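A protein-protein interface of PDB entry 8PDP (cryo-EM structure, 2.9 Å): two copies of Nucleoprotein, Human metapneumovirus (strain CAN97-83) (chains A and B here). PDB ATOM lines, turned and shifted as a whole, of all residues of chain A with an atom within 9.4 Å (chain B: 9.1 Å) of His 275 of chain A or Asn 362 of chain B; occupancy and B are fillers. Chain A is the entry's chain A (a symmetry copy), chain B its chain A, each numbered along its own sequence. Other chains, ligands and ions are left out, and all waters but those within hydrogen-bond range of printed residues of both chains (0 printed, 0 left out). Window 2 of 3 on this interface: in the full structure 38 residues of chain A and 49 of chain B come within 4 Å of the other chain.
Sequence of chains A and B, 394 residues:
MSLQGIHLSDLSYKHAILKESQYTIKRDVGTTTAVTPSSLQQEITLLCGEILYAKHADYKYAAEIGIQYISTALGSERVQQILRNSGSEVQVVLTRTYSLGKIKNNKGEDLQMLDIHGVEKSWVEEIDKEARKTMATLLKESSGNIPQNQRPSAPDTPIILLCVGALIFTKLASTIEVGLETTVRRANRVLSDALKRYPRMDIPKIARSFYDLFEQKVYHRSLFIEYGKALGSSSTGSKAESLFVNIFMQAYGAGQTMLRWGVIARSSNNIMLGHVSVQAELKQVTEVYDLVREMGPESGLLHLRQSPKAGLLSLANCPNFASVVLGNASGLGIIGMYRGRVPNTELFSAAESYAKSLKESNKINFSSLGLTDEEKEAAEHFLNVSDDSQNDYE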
ATOM      1  N   ASN A 270      -6.297  10.594   8.280  1.00  0.00           N
ATOM      2  CA  ASN A 270      -7.636  10.359   7.760  1.00  0.00           C
ATOM      3  C   ASN A 270      -8.353  11.685   7.553  1.00  0.00           C
ATOM      4  O   ASN A 270      -8.507  12.471   8.492  1.00  0.00           O
ATOM      5  CB  ASN A 270      -8.423   9.472   8.723  1.00  0.00           C
ATOM      6  CG  ASN A 270      -9.523   8.696   8.035  1.00  0.00           C
ATOM      7  OD1 ASN A 270      -9.273   7.953   7.089  1.00  0.00           O
ATOM      8  ND2 ASN A 270     -10.751   8.870   8.501  1.00  0.00           N
ATOM      9  N   ILE A 271      -8.782  11.942   6.315  1.00  0.00           N
ATOM     10  CA  ILE A 271      -9.456  13.199   6.017  1.00  0.00           C
ATOM     11  C   ILE A 271     -10.827  13.276   6.669  1.00  0.00           C
ATOM     12  O   ILE A 271     -11.327  14.379   6.920  1.00  0.00           O
ATOM     13  CB  ILE A 271      -9.583  13.408   4.497  1.00  0.00           C
ATOM     14  CG1 ILE A 271     -10.436  12.300   3.875  1.00  0.00           C
ATOM     15  CG2 ILE A 271      -8.208  13.469   3.852  1.00  0.00           C
ATOM     16  CD1 ILE A 271     -10.810  12.550   2.432  1.00  0.00           C
ATOM     17  N   MET A 272     -11.451  12.134   6.963  1.00  0.00           N
ATOM     18  CA  MET A 272     -12.768  12.162   7.582  1.00  0.00           C
ATOM     19  C   MET A 272     -12.720  12.613   9.033  1.00  0.00           C
ATOM     20  O   MET A 272     -13.779  12.819   9.633  1.00  0.00           O
ATOM     21  CB  MET A 272     -13.433  10.791   7.466  1.00  0.00           C
ATOM     22  CG  MET A 272     -13.726  10.400   6.028  1.00  0.00           C
ATOM     23  SD  MET A 272     -14.920  11.520   5.269  1.00  0.00           S
ATOM     24  CE  MET A 272     -14.881  10.973   3.565  1.00  0.00           C
ATOM     25  N   LEU A 273     -11.526  12.760   9.611  1.00  0.00           N
ATOM     26  CA  LEU A 273     -11.405  13.449  10.888  1.00  0.00           C
ATOM     27  C   LEU A 273     -11.788  14.917  10.775  1.00  0.00           C
ATOM     28  O   LEU A 273     -12.173  15.526  11.778  1.00  0.00           O
ATOM     29  CB  LEU A 273      -9.981  13.325  11.427  1.00  0.00           C
ATOM     30  CG  LEU A 273      -9.575  11.952  11.960  1.00  0.00           C
ATOM     31  CD1 LEU A 273      -8.111  11.954  12.360  1.00  0.00           C
ATOM     32  CD2 LEU A 273     -10.454  11.562  13.131  1.00  0.00           C
ATOM     33  N   GLY A 274     -11.695  15.495   9.578  1.00  0.00           N
ATOM     34  CA  GLY A 274     -12.108  16.859   9.334  1.00  0.00           C
ATOM     35  C   GLY A 274     -13.595  17.051   9.176  1.00  0.00           C
ATOM     36  O   GLY A 274     -14.054  18.177   8.972  1.00  0.00           O
ATOM     37  N   HIS A 275     -14.361  15.965   9.261  1.00  0.00           N
ATOM     38  CA  HIS A 275     -15.811  16.048   9.184  1.00  0.00           C
ATOM     39  C   HIS A 275     -16.348  16.903  10.326  1.00  0.00           C
ATOM     40  O   HIS A 275     -15.828  16.871  11.443  1.00  0.00           O
ATOM     41  CB  HIS A 275     -16.405  14.641   9.241  1.00  0.00           C
ATOM     42  CG  HIS A 275     -17.844  14.565   8.849  1.00  0.00           C
ATOM     43  ND1 HIS A 275     -18.870  14.737   9.753  1.00  0.00           N
ATOM     44  CD2 HIS A 275     -18.432  14.310   7.657  1.00  0.00           C
ATOM     45  CE1 HIS A 275     -20.028  14.601   9.133  1.00  0.00           C
ATOM     46  NE2 HIS A 275     -19.790  14.345   7.859  1.00  0.00           N
ATOM     47  N   VAL A 276     -17.396  17.678  10.035  1.00  0.00           N
ATOM     48  CA  VAL A 276     -17.924  18.615  11.027  1.00  0.00           C
ATOM     49  C   VAL A 276     -18.455  17.879  12.248  1.00  0.00           C
ATOM     50  O   VAL A 276     -18.387  18.397  13.369  1.00  0.00           O
ATOM     51  CB  VAL A 276     -19.000  19.519  10.395  1.00  0.00           C
ATOM     52  CG1 VAL A 276     -18.367  20.458   9.385  1.00  0.00           C
ATOM     53  CG2 VAL A 276     -20.089  18.682   9.736  1.00  0.00           C
ATOM     54  N   SER A 277     -18.999  16.675  12.060  1.00  0.00           N
ATOM     55  CA  SER A 277     -19.437  15.883  13.204  1.00  0.00           C
ATOM     56  C   SER A 277     -18.258  15.508  14.093  1.00  0.00           C
ATOM     57  O   SER A 277     -18.367  15.525  15.323  1.00  0.00           O
ATOM     58  CB  SER A 277     -20.169  14.631  12.727  1.00  0.00           C
ATOM     59  OG  SER A 277     -21.358  14.968  12.035  1.00  0.00           O
ATOM     60  N   VAL A 278     -17.122  15.159  13.486  1.00  0.00           N
ATOM     61  CA  VAL A 278     -15.936  14.819  14.264  1.00  0.00           C
ATOM     62  C   VAL A 278     -15.346  16.063  14.917  1.00  0.00           C
ATOM     63  O   VAL A 278     -14.907  16.024  16.072  1.00  0.00           O
ATOM     64  CB  VAL A 278     -14.905  14.105  13.373  1.00  0.00           C
ATOM     65  CG1 VAL A 278     -13.654  13.770  14.168  1.00  0.00           C
ATOM     66  CG2 VAL A 278     -15.516  12.860  12.768  1.00  0.00           C
ATOM     67  N   GLN A 279     -15.320  17.183  14.190  1.00  0.00           N
ATOM     68  CA  GLN A 279     -14.782  18.421  14.744  1.00  0.00           C
ATOM     69  C   GLN A 279     -15.582  18.894  15.950  1.00  0.00           C
ATOM     70  O   GLN A 279     -15.024  19.520  16.857  1.00  0.00           O
ATOM     71  CB  GLN A 279     -14.762  19.511  13.671  1.00  0.00           C
ATOM     72  CG  GLN A 279     -13.825  19.243  12.506  1.00  0.00           C
ATOM     73  CD  GLN A 279     -12.374  19.163  12.929  1.00  0.00           C
ATOM     74  OE1 GLN A 279     -11.763  20.167  13.289  1.00  0.00           O
ATOM     75  NE2 GLN A 279     -11.816  17.959  12.895  1.00  0.00           N
ATOM     76  N   ALA A 280     -16.884  18.613  15.974  1.00  0.00           N
ATOM     77  CA  ALA A 280     -17.739  19.042  17.073  1.00  0.00           C
ATOM     78  C   ALA A 280     -17.451  18.311  18.374  1.00  0.00           C
ATOM     79  O   ALA A 280     -17.962  18.723  19.420  1.00  0.00           O
ATOM     80  CB  ALA A 280     -19.209  18.849  16.699  1.00  0.00           C
ATOM     81  N   GLU A 281     -16.659  17.241  18.339  1.00  0.00           N
ATOM     82  CA  GLU A 281     -16.452  16.404  19.507  1.00  0.00           C
ATOM     83  C   GLU A 281     -14.984  16.277  19.900  1.00  0.00           C
ATOM     84  O   GLU A 281     -14.692  15.758  20.982  1.00  0.00           O
ATOM     85  CB  GLU A 281     -17.059  15.011  19.253  1.00  0.00           C
ATOM     86  CG  GLU A 281     -16.978  14.022  20.401  1.00  0.00           C
ATOM     87  CD  GLU A 281     -17.799  14.460  21.602  1.00  0.00           C
ATOM     88  OE1 GLU A 281     -18.779  15.212  21.412  1.00  0.00           O
ATOM     89  OE2 GLU A 281     -17.468  14.053  22.735  1.00  0.00           O
ATOM     90  N   LEU A 282     -14.057  16.779  19.080  1.00  0.00           N
ATOM     91  CA  LEU A 282     -12.632  16.582  19.330  1.00  0.00           C
ATOM     92  C   LEU A 282     -12.163  17.190  20.644  1.00  0.00           C
ATOM     93  O   LEU A 282     -11.111  16.788  21.155  1.00  0.00           O
ATOM     94  CB  LEU A 282     -11.814  17.166  18.180  1.00  0.00           C
ATOM     95  CG  LEU A 282     -11.629  16.284  16.946  1.00  0.00           C
ATOM     96  CD1 LEU A 282     -10.659  16.932  15.975  1.00  0.00           C
ATOM     97  CD2 LEU A 282     -11.145  14.904  17.345  1.00  0.00           C
ATOM     98  N   ASN A 320     -18.969   9.972  16.799  1.00  0.00           N
ATOM     99  CA  ASN A 320     -18.381  10.320  15.509  1.00  0.00           C
ATOM    100  C   ASN A 320     -16.903   9.959  15.470  1.00  0.00           C
ATOM    101  O   ASN A 320     -16.429   9.330  14.514  1.00  0.00           O
ATOM    102  CB  ASN A 320     -18.572  11.811  15.231  1.00  0.00           C
ATOM    103  CG  ASN A 320     -20.030  12.213  15.174  1.00  0.00           C
ATOM    104  OD1 ASN A 320     -20.833  11.571  14.504  1.00  0.00           O
ATOM    105  ND2 ASN A 320     -20.376  13.288  15.871  1.00  0.00           N
ATOM    106  N   PHE A 321     -16.160  10.347  16.507  1.00  0.00           N
ATOM    107  CA  PHE A 321     -14.739  10.029  16.566  1.00  0.00           C
ATOM    108  C   PHE A 321     -14.519   8.525  16.609  1.00  0.00           C
ATOM    109  O   PHE A 321     -13.638   8.000  15.922  1.00  0.00           O
ATOM    110  CB  PHE A 321     -14.107  10.694  17.788  1.00  0.00           C
ATOM    111  CG  PHE A 321     -12.640  10.426  17.934  1.00  0.00           C
ATOM    112  CD1 PHE A 321     -11.724  11.080  17.134  1.00  0.00           C
ATOM    113  CD2 PHE A 321     -12.178   9.509  18.860  1.00  0.00           C
ATOM    114  CE1 PHE A 321     -10.373  10.835  17.265  1.00  0.00           C
ATOM    115  CE2 PHE A 321     -10.830   9.259  18.991  1.00  0.00           C
ATOM    116  CZ  PHE A 321      -9.927   9.923  18.192  1.00  0.00           C
ATOM    117  N   VAL A 324     -15.215   7.044  13.107  1.00  0.00           N
ATOM    118  CA  VAL A 324     -14.143   7.338  12.160  1.00  0.00           C
ATOM    119  C   VAL A 324     -12.896   6.531  12.494  1.00  0.00           C
ATOM    120  O   VAL A 324     -12.197   6.041  11.597  1.00  0.00           O
ATOM    121  CB  VAL A 324     -13.856   8.848  12.135  1.00  0.00           C
ATOM    122  CG1 VAL A 324     -12.572   9.137  11.382  1.00  0.00           C
ATOM    123  CG2 VAL A 324     -15.019   9.585  11.503  1.00  0.00           C
ATOM    124  N   ASN A 344     -22.008   5.286  13.889  1.00  0.00           N
ATOM    125  CA  ASN A 344     -22.353   5.883  12.603  1.00  0.00           C
ATOM    126  C   ASN A 344     -21.741   5.049  11.486  1.00  0.00           C
ATOM    127  O   ASN A 344     -20.514   4.988  11.347  1.00  0.00           O
ATOM    128  CB  ASN A 344     -21.882   7.332  12.532  1.00  0.00           C
ATOM    129  CG  ASN A 344     -22.544   8.208  13.571  1.00  0.00           C
ATOM    130  OD1 ASN A 344     -22.143   9.349  13.776  1.00  0.00           O
ATOM    131  ND2 ASN A 344     -23.575   7.685  14.221  1.00  0.00           N
ATOM    132  N   GLU A 346     -22.158   5.542   8.168  1.00  0.00           N
ATOM    133  CA  GLU A 346     -21.690   6.351   7.045  1.00  0.00           C
ATOM    134  C   GLU A 346     -20.249   6.803   7.252  1.00  0.00           C
ATOM    135  O   GLU A 346     -19.413   6.684   6.347  1.00  0.00           O
ATOM    136  CB  GLU A 346     -22.605   7.561   6.842  1.00  0.00           C
ATOM    137  CG  GLU A 346     -24.016   7.226   6.379  1.00  0.00           C
ATOM    138  CD  GLU A 346     -24.932   6.833   7.520  1.00  0.00           C
ATOM    139  OE1 GLU A 346     -24.491   6.879   8.687  1.00  0.00           O
ATOM    140  OE2 GLU A 346     -26.100   6.483   7.247  1.00  0.00           O
ATOM    141  N   LEU A 347     -19.941   7.326   8.441  1.00  0.00           N
ATOM    142  CA  LEU A 347     -18.574   7.739   8.738  1.00  0.00           C
ATOM    143  C   LEU A 347     -17.628   6.549   8.720  1.00  0.00           C
ATOM    144  O   LEU A 347     -16.493   6.653   8.241  1.00  0.00           O
ATOM    145  CB  LEU A 347     -18.520   8.442  10.092  1.00  0.00           C
ATOM    146  CG  LEU A 347     -19.255   9.773  10.197  1.00  0.00           C
ATOM    147  CD1 LEU A 347     -19.228  10.271  11.630  1.00  0.00           C
ATOM    148  CD2 LEU A 347     -18.623  10.789   9.261  1.00  0.00           C
ATOM    149  N   PHE A 348     -18.078   5.409   9.243  1.00  0.00           N
ATOM    150  CA  PHE A 348     -17.253   4.207   9.238  1.00  0.00           C
ATOM    151  C   PHE A 348     -16.900   3.798   7.816  1.00  0.00           C
ATOM    152  O   PHE A 348     -15.733   3.530   7.506  1.00  0.00           O
ATOM    153  CB  PHE A 348     -17.993   3.086   9.966  1.00  0.00           C
ATOM    154  CG  PHE A 348     -17.243   1.787  10.025  1.00  0.00           C
ATOM    155  CD1 PHE A 348     -16.379   1.520  11.071  1.00  0.00           C
ATOM    156  CD2 PHE A 348     -17.430   0.816   9.056  1.00  0.00           C
ATOM    157  CE1 PHE A 348     -15.696   0.325  11.136  1.00  0.00           C
ATOM    158  CE2 PHE A 348     -16.750  -0.382   9.118  1.00  0.00           C
ATOM    159  CZ  PHE A 348     -15.883  -0.628  10.160  1.00  0.00           C
ATOM    160  N   ALA A 350     -16.999   5.680   5.032  1.00  0.00           N
ATOM    161  CA  ALA A 350     -16.179   6.688   4.366  1.00  0.00           C
ATOM    162  C   ALA A 350     -14.729   6.618   4.830  1.00  0.00           C
ATOM    163  O   ALA A 350     -13.800   6.692   4.013  1.00  0.00           O
ATOM    164  CB  ALA A 350     -16.755   8.081   4.616  1.00  0.00           C
ATOM    165  N   ALA A 351     -14.517   6.472   6.141  1.00  0.00           N
ATOM    166  CA  ALA A 351     -13.164   6.354   6.665  1.00  0.00           C
ATOM    167  C   ALA A 351     -12.497   5.080   6.170  1.00  0.00           C
ATOM    168  O   ALA A 351     -11.302   5.080   5.860  1.00  0.00           O
ATOM    169  CB  ALA A 351     -13.189   6.393   8.192  1.00  0.00           C
ATOM    170  N   ASN B 269     -21.517  25.288  16.819  1.00  0.00           N
ATOM    171  CA  ASN B 269     -21.379  26.488  15.996  1.00  0.00           C
ATOM    172  C   ASN B 269     -22.737  27.004  15.528  1.00  0.00           C
ATOM    173  O   ASN B 269     -22.901  27.419  14.379  1.00  0.00           O
ATOM    174  CB  ASN B 269     -20.452  26.236  14.805  1.00  0.00           C
ATOM    175  CG  ASN B 269     -19.047  25.859  15.229  1.00  0.00           C
ATOM    176  OD1 ASN B 269     -18.439  26.525  16.066  1.00  0.00           O
ATOM    177  ND2 ASN B 269     -18.524  24.783  14.653  1.00  0.00           N
ATOM    178  N   LYS B 356     -30.893  21.145  12.706  1.00  0.00           N
ATOM    179  CA  LYS B 356     -31.283  20.069  11.804  1.00  0.00           C
ATOM    180  C   LYS B 356     -30.578  20.202  10.462  1.00  0.00           C
ATOM    181  O   LYS B 356     -30.145  19.201   9.880  1.00  0.00           O
ATOM    182  CB  LYS B 356     -32.800  20.045  11.619  1.00  0.00           C
ATOM    183  CG  LYS B 356     -33.563  19.667  12.874  1.00  0.00           C
ATOM    184  CD  LYS B 356     -35.048  19.495  12.602  1.00  0.00           C
ATOM    185  CE  LYS B 356     -35.735  20.832  12.391  1.00  0.00           C
ATOM    186  NZ  LYS B 356     -37.209  20.679  12.235  1.00  0.00           N
ATOM    187  N   SER B 357     -30.441  21.432   9.961  1.00  0.00           N
ATOM    188  CA  SER B 357     -29.706  21.641   8.718  1.00  0.00           C
ATOM    189  C   SER B 357     -28.260  21.178   8.848  1.00  0.00           C
ATOM    190  O   SER B 357     -27.731  20.510   7.952  1.00  0.00           O
ATOM    191  CB  SER B 357     -29.757  23.115   8.323  1.00  0.00           C
ATOM    192  OG  SER B 357     -28.933  23.371   7.200  1.00  0.00           O
ATOM    193  N   LEU B 358     -27.609  21.520   9.960  1.00  0.00           N
ATOM    194  CA  LEU B 358     -26.201  21.176  10.127  1.00  0.00           C
ATOM    195  C   LEU B 358     -26.010  19.675  10.311  1.00  0.00           C
ATOM    196  O   LEU B 358     -25.062  19.095   9.768  1.00  0.00           O
ATOM    197  CB  LEU B 358     -25.612  21.952  11.307  1.00  0.00           C
ATOM    198  CG  LEU B 358     -24.129  21.747  11.613  1.00  0.00           C
ATOM    199  CD1 LEU B 358     -23.444  23.081  11.855  1.00  0.00           C
ATOM    200  CD2 LEU B 358     -23.952  20.837  12.820  1.00  0.00           C
ATOM    201  N   LYS B 359     -26.891  19.028  11.078  1.00  0.00           N
ATOM    202  CA  LYS B 359     -26.743  17.595  11.312  1.00  0.00           C
ATOM    203  C   LYS B 359     -27.081  16.789  10.065  1.00  0.00           C
ATOM    204  O   LYS B 359     -26.368  15.838   9.724  1.00  0.00           O
ATOM    205  CB  LYS B 359     -27.614  17.162  12.493  1.00  0.00           C
ATOM    206  CG  LYS B 359     -27.747  15.656  12.656  1.00  0.00           C
ATOM    207  CD  LYS B 359     -28.693  15.306  13.795  1.00  0.00           C
ATOM    208  CE  LYS B 359     -30.125  15.712  13.497  1.00  0.00           C
ATOM    209  NZ  LYS B 359     -30.759  14.816  12.496  1.00  0.00           N
ATOM    210  N   GLU B 360     -28.161  17.153   9.368  1.00  0.00           N
ATOM    211  CA  GLU B 360     -28.539  16.429   8.158  1.00  0.00           C
ATOM    212  C   GLU B 360     -27.474  16.565   7.078  1.00  0.00           C
ATOM    213  O   GLU B 360     -27.141  15.588   6.396  1.00  0.00           O
ATOM    214  CB  GLU B 360     -29.890  16.930   7.647  1.00  0.00           C
ATOM    215  CG  GLU B 360     -30.454  16.130   6.486  1.00  0.00           C
ATOM    216  CD  GLU B 360     -30.380  14.631   6.712  1.00  0.00           C
ATOM    217  OE1 GLU B 360     -29.873  13.919   5.820  1.00  0.00           O
ATOM    218  OE2 GLU B 360     -30.832  14.167   7.781  1.00  0.00           O
ATOM    219  N   SER B 361     -26.926  17.763   6.911  1.00  0.00           N
ATOM    220  CA  SER B 361     -25.871  17.978   5.937  1.00  0.00           C
ATOM    221  C   SER B 361     -24.537  17.466   6.472  1.00  0.00           C
ATOM    222  O   SER B 361     -24.386  17.152   7.655  1.00  0.00           O
ATOM    223  CB  SER B 361     -25.768  19.460   5.580  1.00  0.00           C
ATOM    224  OG  SER B 361     -27.038  19.996   5.254  1.00  0.00           O
ATOM    225  N   ASN B 362     -23.561  17.376   5.575  1.00  0.00           N
ATOM    226  CA  ASN B 362     -22.206  16.982   5.928  1.00  0.00           C
ATOM    227  C   ASN B 362     -21.211  17.960   5.320  1.00  0.00           C
ATOM    228  O   ASN B 362     -21.451  18.542   4.260  1.00  0.00           O
ATOM    229  CB  ASN B 362     -21.904  15.534   5.486  1.00  0.00           C
ATOM    230  CG  ASN B 362     -22.114  15.309   3.996  1.00  0.00           C
ATOM    231  OD1 ASN B 362     -22.404  16.235   3.240  1.00  0.00           O
ATOM    232  ND2 ASN B 362     -21.967  14.060   3.570  1.00  0.00           N
ATOM    233  N   LYS B 363     -20.095  18.154   6.020  1.00  0.00           N
ATOM    234  CA  LYS B 363     -19.074  19.103   5.604  1.00  0.00           C
ATOM    235  C   LYS B 363     -17.703  18.546   5.953  1.00  0.00           C
ATOM    236  O   LYS B 363     -17.561  17.688   6.827  1.00  0.00           O
ATOM    237  CB  LYS B 363     -19.267  20.475   6.270  1.00  0.00           C
ATOM    238  CG  LYS B 363     -20.468  21.261   5.770  1.00  0.00           C
ATOM    239  CD  LYS B 363     -20.315  21.648   4.310  1.00  0.00           C
ATOM    240  CE  LYS B 363     -21.555  22.367   3.802  1.00  0.00           C
ATOM    241  NZ  LYS B 363     -21.437  22.746   2.367  1.00  0.00           N
ATOM    242  N   ILE B 364     -16.688  19.045   5.252  1.00  0.00           N
ATOM    243  CA  ILE B 364     -15.296  18.691   5.499  1.00  0.00           C
ATOM    244  C   ILE B 364     -14.514  19.973   5.739  1.00  0.00           C
ATOM    245  O   ILE B 364     -14.618  20.925   4.957  1.00  0.00           O
ATOM    246  CB  ILE B 364     -14.689  17.896   4.327  1.00  0.00           C
ATOM    247  CG1 ILE B 364     -15.601  16.730   3.939  1.00  0.00           C
ATOM    248  CG2 ILE B 364     -13.296  17.401   4.687  1.00  0.00           C
ATOM    249  CD1 ILE B 364     -15.760  15.695   5.024  1.00  0.00           C
ATOM    250  N   ASN B 365     -13.738  19.998   6.816  1.00  0.00           N
ATOM    251  CA  ASN B 365     -12.916  21.158   7.136  1.00  0.00           C
ATOM    252  C   ASN B 365     -11.434  20.810   7.065  1.00  0.00           C
ATOM    253  O   ASN B 365     -10.583  21.695   6.980  1.00  0.00           O
ATOM    254  CB  ASN B 365     -13.267  21.701   8.523  1.00  0.00           C
ATOM    255  CG  ASN B 365     -14.763  21.846   8.731  1.00  0.00           C
ATOM    256  OD1 ASN B 365     -15.520  22.025   7.777  1.00  0.00           O
ATOM    257  ND2 ASN B 365     -15.197  21.765   9.983  1.00  0.00           N
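Gly 274 of chain A touches Ile 364 of chain B. His 275 of chain A touches Asn 362 of chain B (NE2 to CB, 3.4 Å). His 275 of chain A touches Lys 363 of chain B. His 275 of chain A touches Ile 364 of chain B. Val 276 of chain A touches Asn 365 of chain B. ND2 of Asn 365 of chain B touches CG of Gln 279 of chain A, 3.8 Å away.
Of the printed residues of chain B, His 275 of chain A touches Asn 362 (3.4 Å), Lys 363 (3.4 Å) and Ile 364 (3.999 Å). Gly 274 of chain A touches two residues of chain B. Val 276 of chain A touches two residues of chain B. No residue of chain B comes within 4 Å of Ser 277 of chain A. No residue of chain B comes within 4 Å of Val 278 of chain A. Of chain A, only His 275 and Val 276 come within 4 Å of Lys 363 of chain B. Of the printed residues of chain A, Asn 365 of chain B touches Gly 274 (2.8 Å), Val 276 (3.5 Å) and Gln 279 (3.8 Å). Of the printed residues of chain B, Gln 279 of chain A touches Asn 365 (3.8 Å). Glu 281 of chain A touches none of the printed residues of chain B. The nearest printed residue of chain B that does not touch His 275 of chain A is Asn 365 of chain B (4.8 Å). The nearest residue of chain A that does not touch Asn 362 of chain B is Val 276 of chain A (4.6 Å). The nearest printed residue of chain A that does not touch Ile 364 of chain B is Ile 271 of chain A (4.2 Å).
The backbone carbonyl oxygen (O) of Leu 273 of chain A lies within hydrogen-bond range of the side-chain amide nitrogen (NE2) of Gln 279 of chain A, 2.7 Å away. ND1 of His 275 of chain A sits at hydrogen-bond distance from N of Ser 277 of chain A, at 3.0 Å.
The backbone carbonyl oxygen (O) of Gly 274 of chain A is in hydrogen-bond range of the backbone NH (N) of Asn 365 of chain B, at 2.8 Å. The backbone carbonyl oxygen (O) of Lys 363 of chain B lies within hydrogen-bond range of the backbone NH (N) of Val 276 of chain A (3.2 Å).
No position is printed for both chains. Of the 8 pairs that touch across the chains among the printed residues, none has its exchanged pair printed and touching as well.
Of the 11 printed residues of chain B, 4 touch a printed residue of chain A. Hydrophobic or aromatic side chains of chain B within 4 Å of the printed part of chain A: Ile 364. Of the 22 printed residues of chain A, 4 touch a printed residue of chain B. Hydrophobic or aromatic side chains of chain A within 4 Å of the printed part of chain B: His 275 and Val 276. Among the printed residues, 8 pairs touch across the chains. Among the printed residues, no Asp or Glu carboxylate lies within 4 Å of a Lys or Arg side-chain nitrogen of the other chain.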
